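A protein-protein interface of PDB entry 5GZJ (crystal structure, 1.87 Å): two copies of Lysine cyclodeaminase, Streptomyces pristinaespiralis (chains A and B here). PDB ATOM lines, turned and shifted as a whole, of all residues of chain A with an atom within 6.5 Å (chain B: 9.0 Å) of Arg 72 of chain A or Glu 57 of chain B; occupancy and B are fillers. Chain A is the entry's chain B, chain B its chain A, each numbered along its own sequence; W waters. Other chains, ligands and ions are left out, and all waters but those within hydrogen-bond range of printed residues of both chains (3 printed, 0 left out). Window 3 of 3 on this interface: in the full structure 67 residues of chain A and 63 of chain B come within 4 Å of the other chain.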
ATOM      1  N   HIS A  48      21.381 -21.571  35.663  1.00  0.00           N
ATOM      2  CA  HIS A  48      20.750 -20.284  35.465  1.00  0.00           C
ATOM      3  C   HIS A  48      19.280 -20.322  35.845  1.00  0.00           C
ATOM      4  O   HIS A  48      18.615 -21.352  35.758  1.00  0.00           O
ATOM      5  CB  HIS A  48      20.863 -19.903  33.996  1.00  0.00           C
ATOM      6  CG  HIS A  48      22.281 -19.720  33.536  1.00  0.00           C
ATOM      7  ND1 HIS A  48      23.029 -20.747  33.004  1.00  0.00           N
ATOM      8  CD2 HIS A  48      23.096 -18.640  33.576  1.00  0.00           C
ATOM      9  CE1 HIS A  48      24.240 -20.307  32.711  1.00  0.00           C
ATOM     10  NE2 HIS A  48      24.306 -19.030  33.049  1.00  0.00           N
ATOM     11  N   SER A  50      15.322 -19.835  35.523  1.00  0.00           N
ATOM     12  CA  SER A  50      14.353 -20.075  34.480  1.00  0.00           C
ATOM     13  C   SER A  50      13.933 -18.800  33.746  1.00  0.00           C
ATOM     14  O   SER A  50      13.970 -17.706  34.322  1.00  0.00           O
ATOM     15  CB  SER A  50      13.101 -20.673  35.176  1.00  0.00           C
ATOM     16  OG  SER A  50      13.451 -21.793  35.926  1.00  0.00           O
ATOM     17  N   PRO A  51      13.535 -18.943  32.490  1.00  0.00           N
ATOM     18  CA  PRO A  51      12.884 -17.804  31.813  1.00  0.00           C
ATOM     19  C   PRO A  51      11.600 -17.405  32.549  1.00  0.00           C
ATOM     20  O   PRO A  51      11.044 -18.230  33.337  1.00  0.00           O
ATOM     21  CB  PRO A  51      12.513 -18.336  30.436  1.00  0.00           C
ATOM     22  CG  PRO A  51      12.805 -19.770  30.429  1.00  0.00           C
ATOM     23  CD  PRO A  51      13.473 -20.183  31.727  1.00  0.00           C
ATOM     24  N   PRO A  70       8.426 -23.018  31.947  1.00  0.00           N
ATOM     25  CA  PRO A  70       9.470 -23.860  31.402  1.00  0.00           C
ATOM     26  C   PRO A  70      10.844 -23.691  32.065  1.00  0.00           C
ATOM     27  O   PRO A  70      11.166 -22.613  32.542  1.00  0.00           O
ATOM     28  CB  PRO A  70       9.573 -23.361  29.940  1.00  0.00           C
ATOM     29  CG  PRO A  70       9.209 -21.928  29.994  1.00  0.00           C
ATOM     30  CD  PRO A  70       8.146 -21.853  31.077  1.00  0.00           C
ATOM     31  N   HIS A  71      11.610 -24.759  32.108  1.00  0.00           N
ATOM     32  CA  HIS A  71      13.006 -24.670  32.539  1.00  0.00           C
ATOM     33  C   HIS A  71      13.764 -25.718  31.750  1.00  0.00           C
ATOM     34  O   HIS A  71      13.435 -26.889  31.803  1.00  0.00           O
ATOM     35  CB  HIS A  71      13.192 -24.962  34.033  1.00  0.00           C
ATOM     36  CG  HIS A  71      14.621 -24.848  34.464  1.00  0.00           C
ATOM     37  ND1 HIS A  71      15.190 -23.635  34.784  1.00  0.00           N
ATOM     38  CD2 HIS A  71      15.611 -25.765  34.526  1.00  0.00           C
ATOM     39  CE1 HIS A  71      16.475 -23.819  35.043  1.00  0.00           C
ATOM     40  NE2 HIS A  71      16.751 -25.100  34.917  1.00  0.00           N
ATOM     41  N   ARG A  72      14.825 -25.305  31.075  1.00  0.00           N
ATOM     42  CA  ARG A  72      15.602 -26.259  30.267  1.00  0.00           C
ATOM     43  C   ARG A  72      16.939 -26.563  30.952  1.00  0.00           C
ATOM     44  O   ARG A  72      17.620 -25.643  31.377  1.00  0.00           O
ATOM     45  CB  ARG A  72      15.873 -25.644  28.928  1.00  0.00           C
ATOM     46  CG  ARG A  72      16.775 -26.413  27.994  1.00  0.00           C
ATOM     47  CD  ARG A  72      16.821 -25.766  26.613  1.00  0.00           C
ATOM     48  NE  ARG A  72      17.660 -26.598  25.736  1.00  0.00           N
ATOM     49  CZ  ARG A  72      18.812 -26.202  25.191  1.00  0.00           C
ATOM     50  NH1 ARG A  72      19.176 -24.945  25.263  1.00  0.00           N
ATOM     51  NH2 ARG A  72      19.528 -27.060  24.483  1.00  0.00           N
ATOM     52  N   GLU A  73      17.310 -27.815  30.904  1.00  0.00           N
ATOM     53  CA  GLU A  73      18.654 -28.287  31.254  1.00  0.00           C
ATOM     54  C   GLU A  73      19.317 -28.806  29.953  1.00  0.00           C
ATOM     55  O   GLU A  73      19.004 -29.874  29.516  1.00  0.00           O
ATOM     56  CB  GLU A  73      18.518 -29.338  32.335  1.00  0.00           C
ATOM     57  CG  GLU A  73      18.281 -28.643  33.700  1.00  0.00           C
ATOM     58  CD  GLU A  73      17.744 -29.524  34.841  1.00  0.00           C
ATOM     59  OE1 GLU A  73      16.558 -29.387  35.278  1.00  0.00           O
ATOM     60  OE2 GLU A  73      18.535 -30.311  35.382  1.00  0.00           O
ATOM     61  N   PRO A  74      20.113 -27.969  29.283  1.00  0.00           N
ATOM     62  CA  PRO A  74      20.574 -28.265  27.905  1.00  0.00           C
ATOM     63  C   PRO A  74      21.226 -29.608  27.771  1.00  0.00           C
ATOM     64  O   PRO A  74      22.077 -30.006  28.600  1.00  0.00           O
ATOM     65  CB  PRO A  74      21.528 -27.116  27.599  1.00  0.00           C
ATOM     66  CG  PRO A  74      21.037 -26.015  28.457  1.00  0.00           C
ATOM     67  CD  PRO A  74      20.562 -26.647  29.718  1.00  0.00           C
ATOM     68  N   GLY A  75      20.789 -30.367  26.782  1.00  0.00           N
ATOM     69  CA  GLY A  75      21.363 -31.668  26.557  1.00  0.00           C
ATOM     70  C   GLY A  75      20.683 -32.740  27.362  1.00  0.00           C
ATOM     71  O   GLY A  75      20.890 -33.901  27.128  1.00  0.00           O
ATOM     72  N   HIS A  77      16.983 -32.422  29.552  1.00  0.00           N
ATOM     73  CA  HIS A  77      15.492 -32.333  29.447  1.00  0.00           C
ATOM     74  C   HIS A  77      14.971 -30.952  29.748  1.00  0.00           C
ATOM     75  O   HIS A  77      15.690 -30.061  30.252  1.00  0.00           O
ATOM     76  CB  HIS A  77      14.817 -33.363  30.349  1.00  0.00           C
ATOM     77  CG  HIS A  77      15.315 -33.340  31.752  1.00  0.00           C
ATOM     78  ND1 HIS A  77      14.874 -32.424  32.685  1.00  0.00           N
ATOM     79  CD2 HIS A  77      16.249 -34.098  32.380  1.00  0.00           C
ATOM     80  CE1 HIS A  77      15.508 -32.628  33.831  1.00  0.00           C
ATOM     81  NE2 HIS A  77      16.342 -33.634  33.670  1.00  0.00           N
ATOM     82  N   ILE A  78      13.718 -30.764  29.364  1.00  0.00           N
ATOM     83  CA  ILE A  78      12.947 -29.548  29.586  1.00  0.00           C
ATOM     84  C   ILE A  78      11.815 -29.940  30.512  1.00  0.00           C
ATOM     85  O   ILE A  78      11.165 -30.950  30.308  1.00  0.00           O
ATOM     86  CB  ILE A  78      12.383 -28.987  28.270  1.00  0.00           C
ATOM     87  CG1 ILE A  78      13.497 -28.533  27.356  1.00  0.00           C
ATOM     88  CG2 ILE A  78      11.434 -27.795  28.488  1.00  0.00           C
ATOM     89  CD1 ILE A  78      13.068 -28.292  25.944  1.00  0.00           C
ATOM     90  N   THR A  79      11.642 -29.156  31.559  1.00  0.00           N
ATOM     91  CA  THR A  79      10.503 -29.314  32.464  1.00  0.00           C
ATOM     92  C   THR A  79       9.473 -28.227  32.127  1.00  0.00           C
ATOM     93  O   THR A  79       9.854 -27.052  31.890  1.00  0.00           O
ATOM     94  CB  THR A  79      10.976 -29.110  33.915  1.00  0.00           C
ATOM     95  OG1 THR A  79      12.002 -30.082  34.272  1.00  0.00           O
ATOM     96  CG2 THR A  79       9.846 -29.268  34.871  1.00  0.00           C
ATOM     97  N   ASP A 107      15.360 -33.249  25.916  1.00  0.00           N
ATOM     98  CA  ASP A 107      15.965 -32.088  25.202  1.00  0.00           C
ATOM     99  C   ASP A 107      16.518 -32.385  23.809  1.00  0.00           C
ATOM    100  O   ASP A 107      16.607 -31.497  22.923  1.00  0.00           O
ATOM    101  CB  ASP A 107      17.044 -31.384  26.024  1.00  0.00           C
ATOM    102  CG  ASP A 107      17.414 -30.022  25.465  1.00  0.00           C
ATOM    103  OD1 ASP A 107      16.522 -29.090  25.335  1.00  0.00           O
ATOM    104  OD2 ASP A 107      18.624 -29.834  25.158  1.00  0.00           O
ATOM    105  N   GLY B  54       5.795 -19.311  22.116  1.00  0.00           N
ATOM    106  CA  GLY B  54       7.126 -19.096  22.634  1.00  0.00           C
ATOM    107  C   GLY B  54       7.865 -20.372  22.491  1.00  0.00           C
ATOM    108  O   GLY B  54       7.264 -21.407  22.185  1.00  0.00           O
ATOM    109  N   GLY B  55       9.182 -20.318  22.696  1.00  0.00           N
ATOM    110  CA  GLY B  55       9.928 -21.531  22.729  1.00  0.00           C
ATOM    111  C   GLY B  55      11.336 -21.373  23.231  1.00  0.00           C
ATOM    112  O   GLY B  55      11.783 -20.268  23.522  1.00  0.00           O
ATOM    113  N   LEU B  56      11.990 -22.516  23.342  1.00  0.00           N
ATOM    114  CA  LEU B  56      13.392 -22.595  23.761  1.00  0.00           C
ATOM    115  C   LEU B  56      14.203 -23.139  22.625  1.00  0.00           C
ATOM    116  O   LEU B  56      13.980 -24.282  22.203  1.00  0.00           O
ATOM    117  CB  LEU B  56      13.522 -23.471  24.988  1.00  0.00           C
ATOM    118  CG  LEU B  56      12.690 -23.042  26.192  1.00  0.00           C
ATOM    119  CD1 LEU B  56      12.544 -24.199  27.138  1.00  0.00           C
ATOM    120  CD2 LEU B  56      13.305 -21.836  26.816  1.00  0.00           C
ATOM    121  N   GLU B  57      15.197 -22.342  22.188  1.00  0.00           N
ATOM    122  CA  GLU B  57      16.075 -22.760  21.095  1.00  0.00           C
ATOM    123  C   GLU B  57      17.056 -23.791  21.614  1.00  0.00           C
ATOM    124  O   GLU B  57      17.517 -23.698  22.756  1.00  0.00           O
ATOM    125  CB  GLU B  57      16.797 -21.567  20.454  1.00  0.00           C
ATOM    126  CG  GLU B  57      15.836 -20.526  19.936  1.00  0.00           C
ATOM    127  CD  GLU B  57      16.528 -19.332  19.263  1.00  0.00           C
ATOM    128  OE1 GLU B  57      17.681 -19.058  19.583  1.00  0.00           O
ATOM    129  OE2 GLU B  57      15.903 -18.634  18.439  1.00  0.00           O
ATOM    130  N   ARG B  58      17.330 -24.816  20.818  1.00  0.00           N
ATOM    131  CA  ARG B  58      18.264 -25.858  21.182  1.00  0.00           C
ATOM    132  C   ARG B  58      19.274 -25.959  20.050  1.00  0.00           C
ATOM    133  O   ARG B  58      18.878 -26.121  18.898  1.00  0.00           O
ATOM    134  CB  ARG B  58      17.555 -27.177  21.373  1.00  0.00           C
ATOM    135  CG  ARG B  58      16.451 -27.141  22.430  1.00  0.00           C
ATOM    136  CD  ARG B  58      15.172 -27.730  21.942  1.00  0.00           C
ATOM    137  NE  ARG B  58      15.217 -29.149  21.781  1.00  0.00           N
ATOM    138  CZ  ARG B  58      14.813 -29.828  20.726  1.00  0.00           C
ATOM    139  NH1 ARG B  58      14.932 -31.095  20.727  1.00  0.00           N
ATOM    140  NH2 ARG B  58      14.271 -29.249  19.648  1.00  0.00           N
ATOM    141  N   SER B  59      20.562 -25.830  20.371  1.00  0.00           N
ATOM    142  CA  SER B  59      21.613 -25.799  19.333  1.00  0.00           C
ATOM    143  C   SER B  59      21.985 -27.166  18.852  1.00  0.00           C
ATOM    144  O   SER B  59      22.438 -27.318  17.743  1.00  0.00           O
ATOM    145  CB  SER B  59      22.850 -25.007  19.836  1.00  0.00           C
ATOM    146  OG  SER B  59      22.595 -23.574  19.852  1.00  0.00           O
ATOM    147  N   GLU B  60      21.764 -28.169  19.675  1.00  0.00           N
ATOM    148  CA  GLU B  60      22.229 -29.512  19.410  1.00  0.00           C
ATOM    149  C   GLU B  60      21.070 -30.538  19.372  1.00  0.00           C
ATOM    150  O   GLU B  60      20.071 -30.324  20.012  1.00  0.00           O
ATOM    151  CB  GLU B  60      23.315 -29.911  20.428  1.00  0.00           C
ATOM    152  CG  GLU B  60      24.651 -29.189  20.130  1.00  0.00           C
ATOM    153  CD  GLU B  60      25.798 -29.642  21.033  1.00  0.00           C
ATOM    154  OE1 GLU B  60      25.944 -30.876  21.230  1.00  0.00           O
ATOM    155  OE2 GLU B  60      26.548 -28.767  21.541  1.00  0.00           O
ATOM    156  N   PRO B  61      21.177 -31.620  18.608  1.00  0.00           N
ATOM    157  CA  PRO B  61      22.385 -31.958  17.796  1.00  0.00           C
ATOM    158  C   PRO B  61      22.603 -30.964  16.665  1.00  0.00           C
ATOM    159  O   PRO B  61      23.722 -30.476  16.450  1.00  0.00           O
ATOM    160  CB  PRO B  61      22.099 -33.370  17.280  1.00  0.00           C
ATOM    161  CG  PRO B  61      20.780 -33.800  17.831  1.00  0.00           C
ATOM    162  CD  PRO B  61      20.238 -32.759  18.762  1.00  0.00           C
ATOM    163  N   VAL B  62      21.506 -30.591  16.017  1.00  0.00           N
ATOM    164  CA  VAL B  62      21.499 -29.554  15.028  1.00  0.00           C
ATOM    165  C   VAL B  62      20.446 -28.557  15.533  1.00  0.00           C
ATOM    166  O   VAL B  62      19.590 -28.909  16.355  1.00  0.00           O
ATOM    167  CB  VAL B  62      21.108 -30.140  13.629  1.00  0.00           C
ATOM    168  CG1 VAL B  62      22.003 -31.329  13.227  1.00  0.00           C
ATOM    169  CG2 VAL B  62      19.724 -30.678  13.633  1.00  0.00           C
ATOM    170  N   PRO B  63      20.501 -27.332  15.059  1.00  0.00           N
ATOM    171  CA  PRO B  63      19.628 -26.366  15.672  1.00  0.00           C
ATOM    172  C   PRO B  63      18.128 -26.662  15.523  1.00  0.00           C
ATOM    173  O   PRO B  63      17.632 -26.939  14.428  1.00  0.00           O
ATOM    174  CB  PRO B  63      19.976 -25.086  14.977  1.00  0.00           C
ATOM    175  CG  PRO B  63      21.417 -25.249  14.614  1.00  0.00           C
ATOM    176  CD  PRO B  63      21.676 -26.697  14.405  1.00  0.00           C
ATOM    177  N   GLY B  64      17.419 -26.515  16.625  1.00  0.00           N
ATOM    178  CA  GLY B  64      15.965 -26.765  16.641  1.00  0.00           C
ATOM    179  C   GLY B  64      15.345 -25.947  17.742  1.00  0.00           C
ATOM    180  O   GLY B  64      15.964 -24.994  18.266  1.00  0.00           O
ATOM    181  N   ILE B  65      14.071 -26.242  18.045  1.00  0.00           N
ATOM    182  CA  ILE B  65      13.323 -25.399  18.968  1.00  0.00           C
ATOM    183  C   ILE B  65      12.251 -26.276  19.645  1.00  0.00           C
ATOM    184  O   ILE B  65      11.832 -27.249  19.084  1.00  0.00           O
ATOM    185  CB  ILE B  65      12.784 -24.134  18.310  1.00  0.00           C
ATOM    186  CG1 ILE B  65      12.293 -23.154  19.371  1.00  0.00           C
ATOM    187  CG2 ILE B  65      11.618 -24.447  17.317  1.00  0.00           C
ATOM    188  CD1 ILE B  65      11.965 -21.762  18.853  1.00  0.00           C
ATOM    189  N   TRP B  66      11.929 -25.990  20.886  1.00  0.00           N
ATOM    190  CA  TRP B  66      10.780 -26.641  21.563  1.00  0.00           C
ATOM    191  C   TRP B  66       9.851 -25.523  21.972  1.00  0.00           C
ATOM    192  O   TRP B  66      10.292 -24.551  22.602  1.00  0.00           O
ATOM    193  CB  TRP B  66      11.259 -27.479  22.739  1.00  0.00           C
ATOM    194  CG  TRP B  66      10.162 -28.150  23.441  1.00  0.00           C
ATOM    195  CD1 TRP B  66       9.581 -29.347  23.141  1.00  0.00           C
ATOM    196  CD2 TRP B  66       9.437 -27.619  24.558  1.00  0.00           C
ATOM    197  NE1 TRP B  66       8.573 -29.596  24.017  1.00  0.00           N
ATOM    198  CE2 TRP B  66       8.476 -28.584  24.918  1.00  0.00           C
ATOM    199  CE3 TRP B  66       9.548 -26.454  25.303  1.00  0.00           C
ATOM    200  CZ2 TRP B  66       7.588 -28.392  26.004  1.00  0.00           C
ATOM    201  CZ3 TRP B  66       8.658 -26.247  26.409  1.00  0.00           C
ATOM    202  CH2 TRP B  66       7.705 -27.213  26.714  1.00  0.00           C
ATOM    203  N   GLU B  67       8.591 -25.619  21.568  1.00  0.00           N
ATOM    204  CA  GLU B  67       7.673 -24.494  21.639  1.00  0.00           C
ATOM    205  C   GLU B  67       6.417 -24.869  22.432  1.00  0.00           C
ATOM    206  O   GLU B  67       6.007 -26.048  22.467  1.00  0.00           O
ATOM    207  CB  GLU B  67       7.285 -24.029  20.239  1.00  0.00           C
ATOM    208  CG  GLU B  67       8.436 -23.351  19.506  1.00  0.00           C
ATOM    209  CD  GLU B  67       8.147 -23.019  18.026  1.00  0.00           C
ATOM    210  OE1 GLU B  67       7.491 -23.809  17.315  1.00  0.00           O
ATOM    211  OE2 GLU B  67       8.635 -21.982  17.573  1.00  0.00           O
ATOM    212  N   TRP B  68       5.778 -23.838  22.964  1.00  0.00           N
ATOM    213  CA  TRP B  68       4.488 -23.936  23.614  1.00  0.00           C
ATOM    214  C   TRP B  68       3.539 -22.969  22.917  1.00  0.00           C
ATOM    215  O   TRP B  68       3.941 -21.857  22.535  1.00  0.00           O
ATOM    216  CB  TRP B  68       4.586 -23.645  25.121  1.00  0.00           C
ATOM    217  CG  TRP B  68       5.291 -22.346  25.478  1.00  0.00           C
ATOM    218  CD1 TRP B  68       4.754 -21.119  25.521  1.00  0.00           C
ATOM    219  CD2 TRP B  68       6.698 -22.173  25.738  1.00  0.00           C
ATOM    220  NE1 TRP B  68       5.738 -20.176  25.768  1.00  0.00           N
ATOM    221  CE2 TRP B  68       6.928 -20.817  25.953  1.00  0.00           C
ATOM    222  CE3 TRP B  68       7.769 -23.037  25.798  1.00  0.00           C
ATOM    223  CZ2 TRP B  68       8.196 -20.302  26.233  1.00  0.00           C
ATOM    224  CZ3 TRP B  68       9.020 -22.521  26.104  1.00  0.00           C
ATOM    225  CH2 TRP B  68       9.217 -21.180  26.328  1.00  0.00           C
ATOM    226  N   TYR B  85      10.699 -29.234  17.338  1.00  0.00           N
ATOM    227  CA  TYR B  85      11.235 -29.321  15.960  1.00  0.00           C
ATOM    228  C   TYR B  85      12.713 -29.711  16.163  1.00  0.00           C
ATOM    229  O   TYR B  85      13.471 -28.928  16.768  1.00  0.00           O
ATOM    230  CB  TYR B  85      11.152 -27.964  15.331  1.00  0.00           C
ATOM    231  CG  TYR B  85      12.015 -27.783  14.092  1.00  0.00           C
ATOM    232  CD1 TYR B  85      11.668 -28.402  12.926  1.00  0.00           C
ATOM    233  CD2 TYR B  85      13.154 -26.992  14.100  1.00  0.00           C
ATOM    234  CE1 TYR B  85      12.418 -28.262  11.767  1.00  0.00           C
ATOM    235  CE2 TYR B  85      13.960 -26.858  12.949  1.00  0.00           C
ATOM    236  CZ  TYR B  85      13.566 -27.478  11.779  1.00  0.00           C
ATOM    237  OH  TYR B  85      14.278 -27.339  10.597  1.00  0.00           O
ATOM    238  N   VAL B 217      18.480 -21.781   9.360  1.00  0.00           N
ATOM    239  CA  VAL B 217      18.631 -20.321   9.291  1.00  0.00           C
ATOM    240  C   VAL B 217      19.881 -20.044   8.409  1.00  0.00           C
ATOM    241  O   VAL B 217      20.928 -20.690   8.598  1.00  0.00           O
ATOM    242  CB  VAL B 217      18.770 -19.726  10.700  1.00  0.00           C
ATOM    243  CG1 VAL B 217      19.046 -18.242  10.631  1.00  0.00           C
ATOM    244  CG2 VAL B 217      17.496 -19.999  11.492  1.00  0.00           C
ATOM    245  N   ASP B 240      10.067 -22.506  12.060  1.00  0.00           N
ATOM    246  CA  ASP B 240      10.624 -23.034  13.267  1.00  0.00           C
ATOM    247  C   ASP B 240      11.343 -21.988  14.016  1.00  0.00           C
ATOM    248  O   ASP B 240      10.792 -21.409  14.953  1.00  0.00           O
ATOM    249  CB  ASP B 240      11.484 -24.318  13.014  1.00  0.00           C
ATOM    250  CG  ASP B 240      12.329 -24.226  11.715  1.00  0.00           C
ATOM    251  OD1 ASP B 240      13.352 -23.522  11.744  1.00  0.00           O
ATOM    252  OD2 ASP B 240      11.975 -24.898  10.733  1.00  0.00           O
ATOM    253  N   LEU B 241      12.576 -21.670  13.581  1.00  0.00           N
ATOM    254  CA  LEU B 241      13.385 -20.731  14.288  1.00  0.00           C
ATOM    255  C   LEU B 241      13.223 -19.326  13.745  1.00  0.00           C
ATOM    256  O   LEU B 241      13.058 -19.110  12.543  1.00  0.00           O
ATOM    257  CB  LEU B 241      14.846 -21.169  14.144  1.00  0.00           C
ATOM    258  CG  LEU B 241      15.222 -22.439  14.909  1.00  0.00           C
ATOM    259  CD1 LEU B 241      16.446 -23.118  14.286  1.00  0.00           C
ATOM    260  CD2 LEU B 241      15.504 -22.018  16.353  1.00  0.00           C
ATOM    261  N   VAL B 242      13.416 -18.352  14.623  1.00  0.00           N
ATOM    262  CA  VAL B 242      13.528 -16.978  14.164  1.00  0.00           C
ATOM    263  C   VAL B 242      14.740 -16.899  13.232  1.00  0.00           C
ATOM    264  O   VAL B 242      15.802 -17.410  13.577  1.00  0.00           O
ATOM    265  CB  VAL B 242      13.689 -16.014  15.346  1.00  0.00           C
ATOM    266  CG1 VAL B 242      14.102 -14.642  14.893  1.00  0.00           C
ATOM    267  CG2 VAL B 242      12.435 -15.981  16.207  1.00  0.00           C
ATOM    268  N   GLY B 243      14.564 -16.283  12.089  1.00  0.00           N
ATOM    269  CA  GLY B 243      15.559 -16.221  11.034  1.00  0.00           C
ATOM    270  C   GLY B 243      15.339 -17.159   9.872  1.00  0.00           C
ATOM    271  O   GLY B 243      15.879 -16.960   8.771  1.00  0.00           O
ATOM    272  N   LYS B 244      14.532 -18.180  10.070  1.00  0.00           N
ATOM    273  CA  LYS B 244      14.334 -19.195   9.053  1.00  0.00           C
ATOM    274  C   LYS B 244      13.268 -18.797   8.026  1.00  0.00           C
ATOM    275  O   LYS B 244      12.141 -18.449   8.394  1.00  0.00           O
ATOM    276  CB  LYS B 244      13.975 -20.549   9.674  1.00  0.00           C
ATOM    277  CG  LYS B 244      13.745 -21.683   8.672  1.00  0.00           C
ATOM    278  CD  LYS B 244      12.294 -22.173   8.608  1.00  0.00           C
ATOM    279  CE  LYS B 244      12.103 -23.327   7.673  1.00  0.00           C
ATOM    280  NZ  LYS B 244      12.765 -24.543   8.166  1.00  0.00           N
ATOM    281  N   ARG B 267       7.387 -12.668  12.901  1.00  0.00           N
ATOM    282  CA  ARG B 267       8.497 -13.196  13.666  1.00  0.00           C
ATOM    283  C   ARG B 267       9.101 -14.491  13.154  1.00  0.00           C
ATOM    284  O   ARG B 267      10.307 -14.674  13.252  1.00  0.00           O
ATOM    285  CB  ARG B 267       8.060 -13.372  15.105  1.00  0.00           C
ATOM    286  CG  ARG B 267       7.771 -12.051  15.751  1.00  0.00           C
ATOM    287  CD  ARG B 267       7.104 -12.289  17.081  1.00  0.00           C
ATOM    288  NE  ARG B 267       6.873 -11.051  17.829  1.00  0.00           N
ATOM    289  CZ  ARG B 267       6.120 -10.021  17.428  1.00  0.00           C
ATOM    290  NH1 ARG B 267       5.490 -10.014  16.236  1.00  0.00           N
ATOM    291  NH2 ARG B 267       5.992  -8.979  18.238  1.00  0.00           N
ATOM    292  N   GLU B 268       8.279 -15.406  12.643  1.00  0.00           N
ATOM    293  CA  GLU B 268       8.755 -16.747  12.267  1.00  0.00           C
ATOM    294  C   GLU B 268       8.368 -17.269  10.912  1.00  0.00           C
ATOM    295  O   GLU B 268       8.724 -18.372  10.536  1.00  0.00           O
ATOM    296  CB  GLU B 268       8.182 -17.708  13.301  1.00  0.00           C
ATOM    297  CG  GLU B 268       8.825 -17.570  14.624  1.00  0.00           C
ATOM    298  CD  GLU B 268       8.215 -18.454  15.703  1.00  0.00           C
ATOM    299  OE1 GLU B 268       7.978 -19.667  15.456  1.00  0.00           O
ATOM    300  OE2 GLU B 268       8.052 -17.935  16.831  1.00  0.00           O
HETATM  301  O   HOH W   1      19.641 -30.410  22.567  1.00  0.00           O
HETATM  302  O   HOH W   2      21.693 -24.910  23.102  1.00  0.00           O
HETATM  303  O   HOH W   3      17.339 -22.141  24.993  1.00  0.00           O
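No position is printed for both chains. Of the 6 pairs that touch across the chains among the printed residues, none has its exchanged pair printed and touching as well.
O of Glu 57 of chain B is in hydrogen-bond range of NH1 of Arg 72 of chain A, 3.3 Å away. The guanidinium group (NE) of Arg 58 of chain B is in salt-bridge range of the side-chain carboxylate (OD1) of Asp 107 of chain A, at 3.8 Å.
Arg 72 of chain A touches two residues of chain B. Glu 57 of chain B touches one residue of chain A. Of the printed residues of chain B, Ile 78 of chain A touches Leu 56 (3.998 Å) and Trp 66 (3.8 Å). Printed residues of chain A within 4 Å of Arg 58 of chain B: Arg 72 and Asp 107. Of the printed residues of chain A, Leu 56 of chain B touches Ile 78 (3.998 Å). Of the printed residues of chain B, Pro 70 of chain A touches Trp 68. Printed residues of chain B within 4 Å of Asp 107 of chain A: Arg 58. Glu 60 of chain B touches none of the printed residues of chain A. The nearest residue of chain B that does not touch Arg 72 of chain A is Leu 56 of chain B (4.05 Å). The nearest residue of chain A that does not touch Glu 57 of chain B is Asp 107 of chain A (6.1 Å).
Hydrophobic or aromatic side chains of chain B that line the printed part of chain A: Leu 56, Trp 66 and Trp 68. Among the printed residues, 6 pairs touch across the chains. Among the printed residues, Asp or Glu carboxylates within 4 Å of a Lys or Arg side-chain nitrogen of the other chain: Asp 107 of chain A with Arg 58 of chain B (3.8 Å).
Trp 68 of chain B touches Pro 70 of chain A (CH2 to CG, 3.7 Å). Arg 72 of chain A touches Arg 58 of chain B (NE to CG, 3.6 Å). Ile 78 of chain A touches Leu 56 of chain B (CG2 to CD1, 3.998 Å). Trp 66 of chain B touches Ile 78 of chain A.
Water W1 bridges O of Glu 60 of chain B (2.6 Å) and OD2 of Asp 107 of chain A (2.8 Å). Water W3 bridges the backbone carbonyl oxygen of Glu 57 of chain B (2.7 Å) and the guanidinium group of Arg 72 of chain A (3.4 Å). Water W2 bridges the backbone NH (N) of Ser 59 of chain B (3.1 Å) and the guanidinium group (NH1) of Arg 72 of chain A (3.3 Å).
The backbone carbonyl oxygen (O) of Gly 54 of chain B sits at hydrogen-bond distance from the backbone NH (N) of Trp 68 of chain B (3.0 Å). O of Arg 58 of chain B sits at hydrogen-bond distance from N of Gly 64 of chain B (2.7 Å). NH2 of Arg 58 of chain B sits at hydrogen-bond distance from O of Ile 65 of chain B (3.2 Å). The guanidinium group of Arg 58 of chain B sits at hydrogen-bond distance from the backbone carbonyl oxygen of Tyr 85 of chain B (3.0 Å). NE of Arg 72 of chain A lies within salt-bridge range of OD1 of Asp 107 of chain A (2.8 Å). OD2 of Asp 107 of chain A is in hydrogen-bond range of N of Gly 75 of chain A (2.8 Å).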
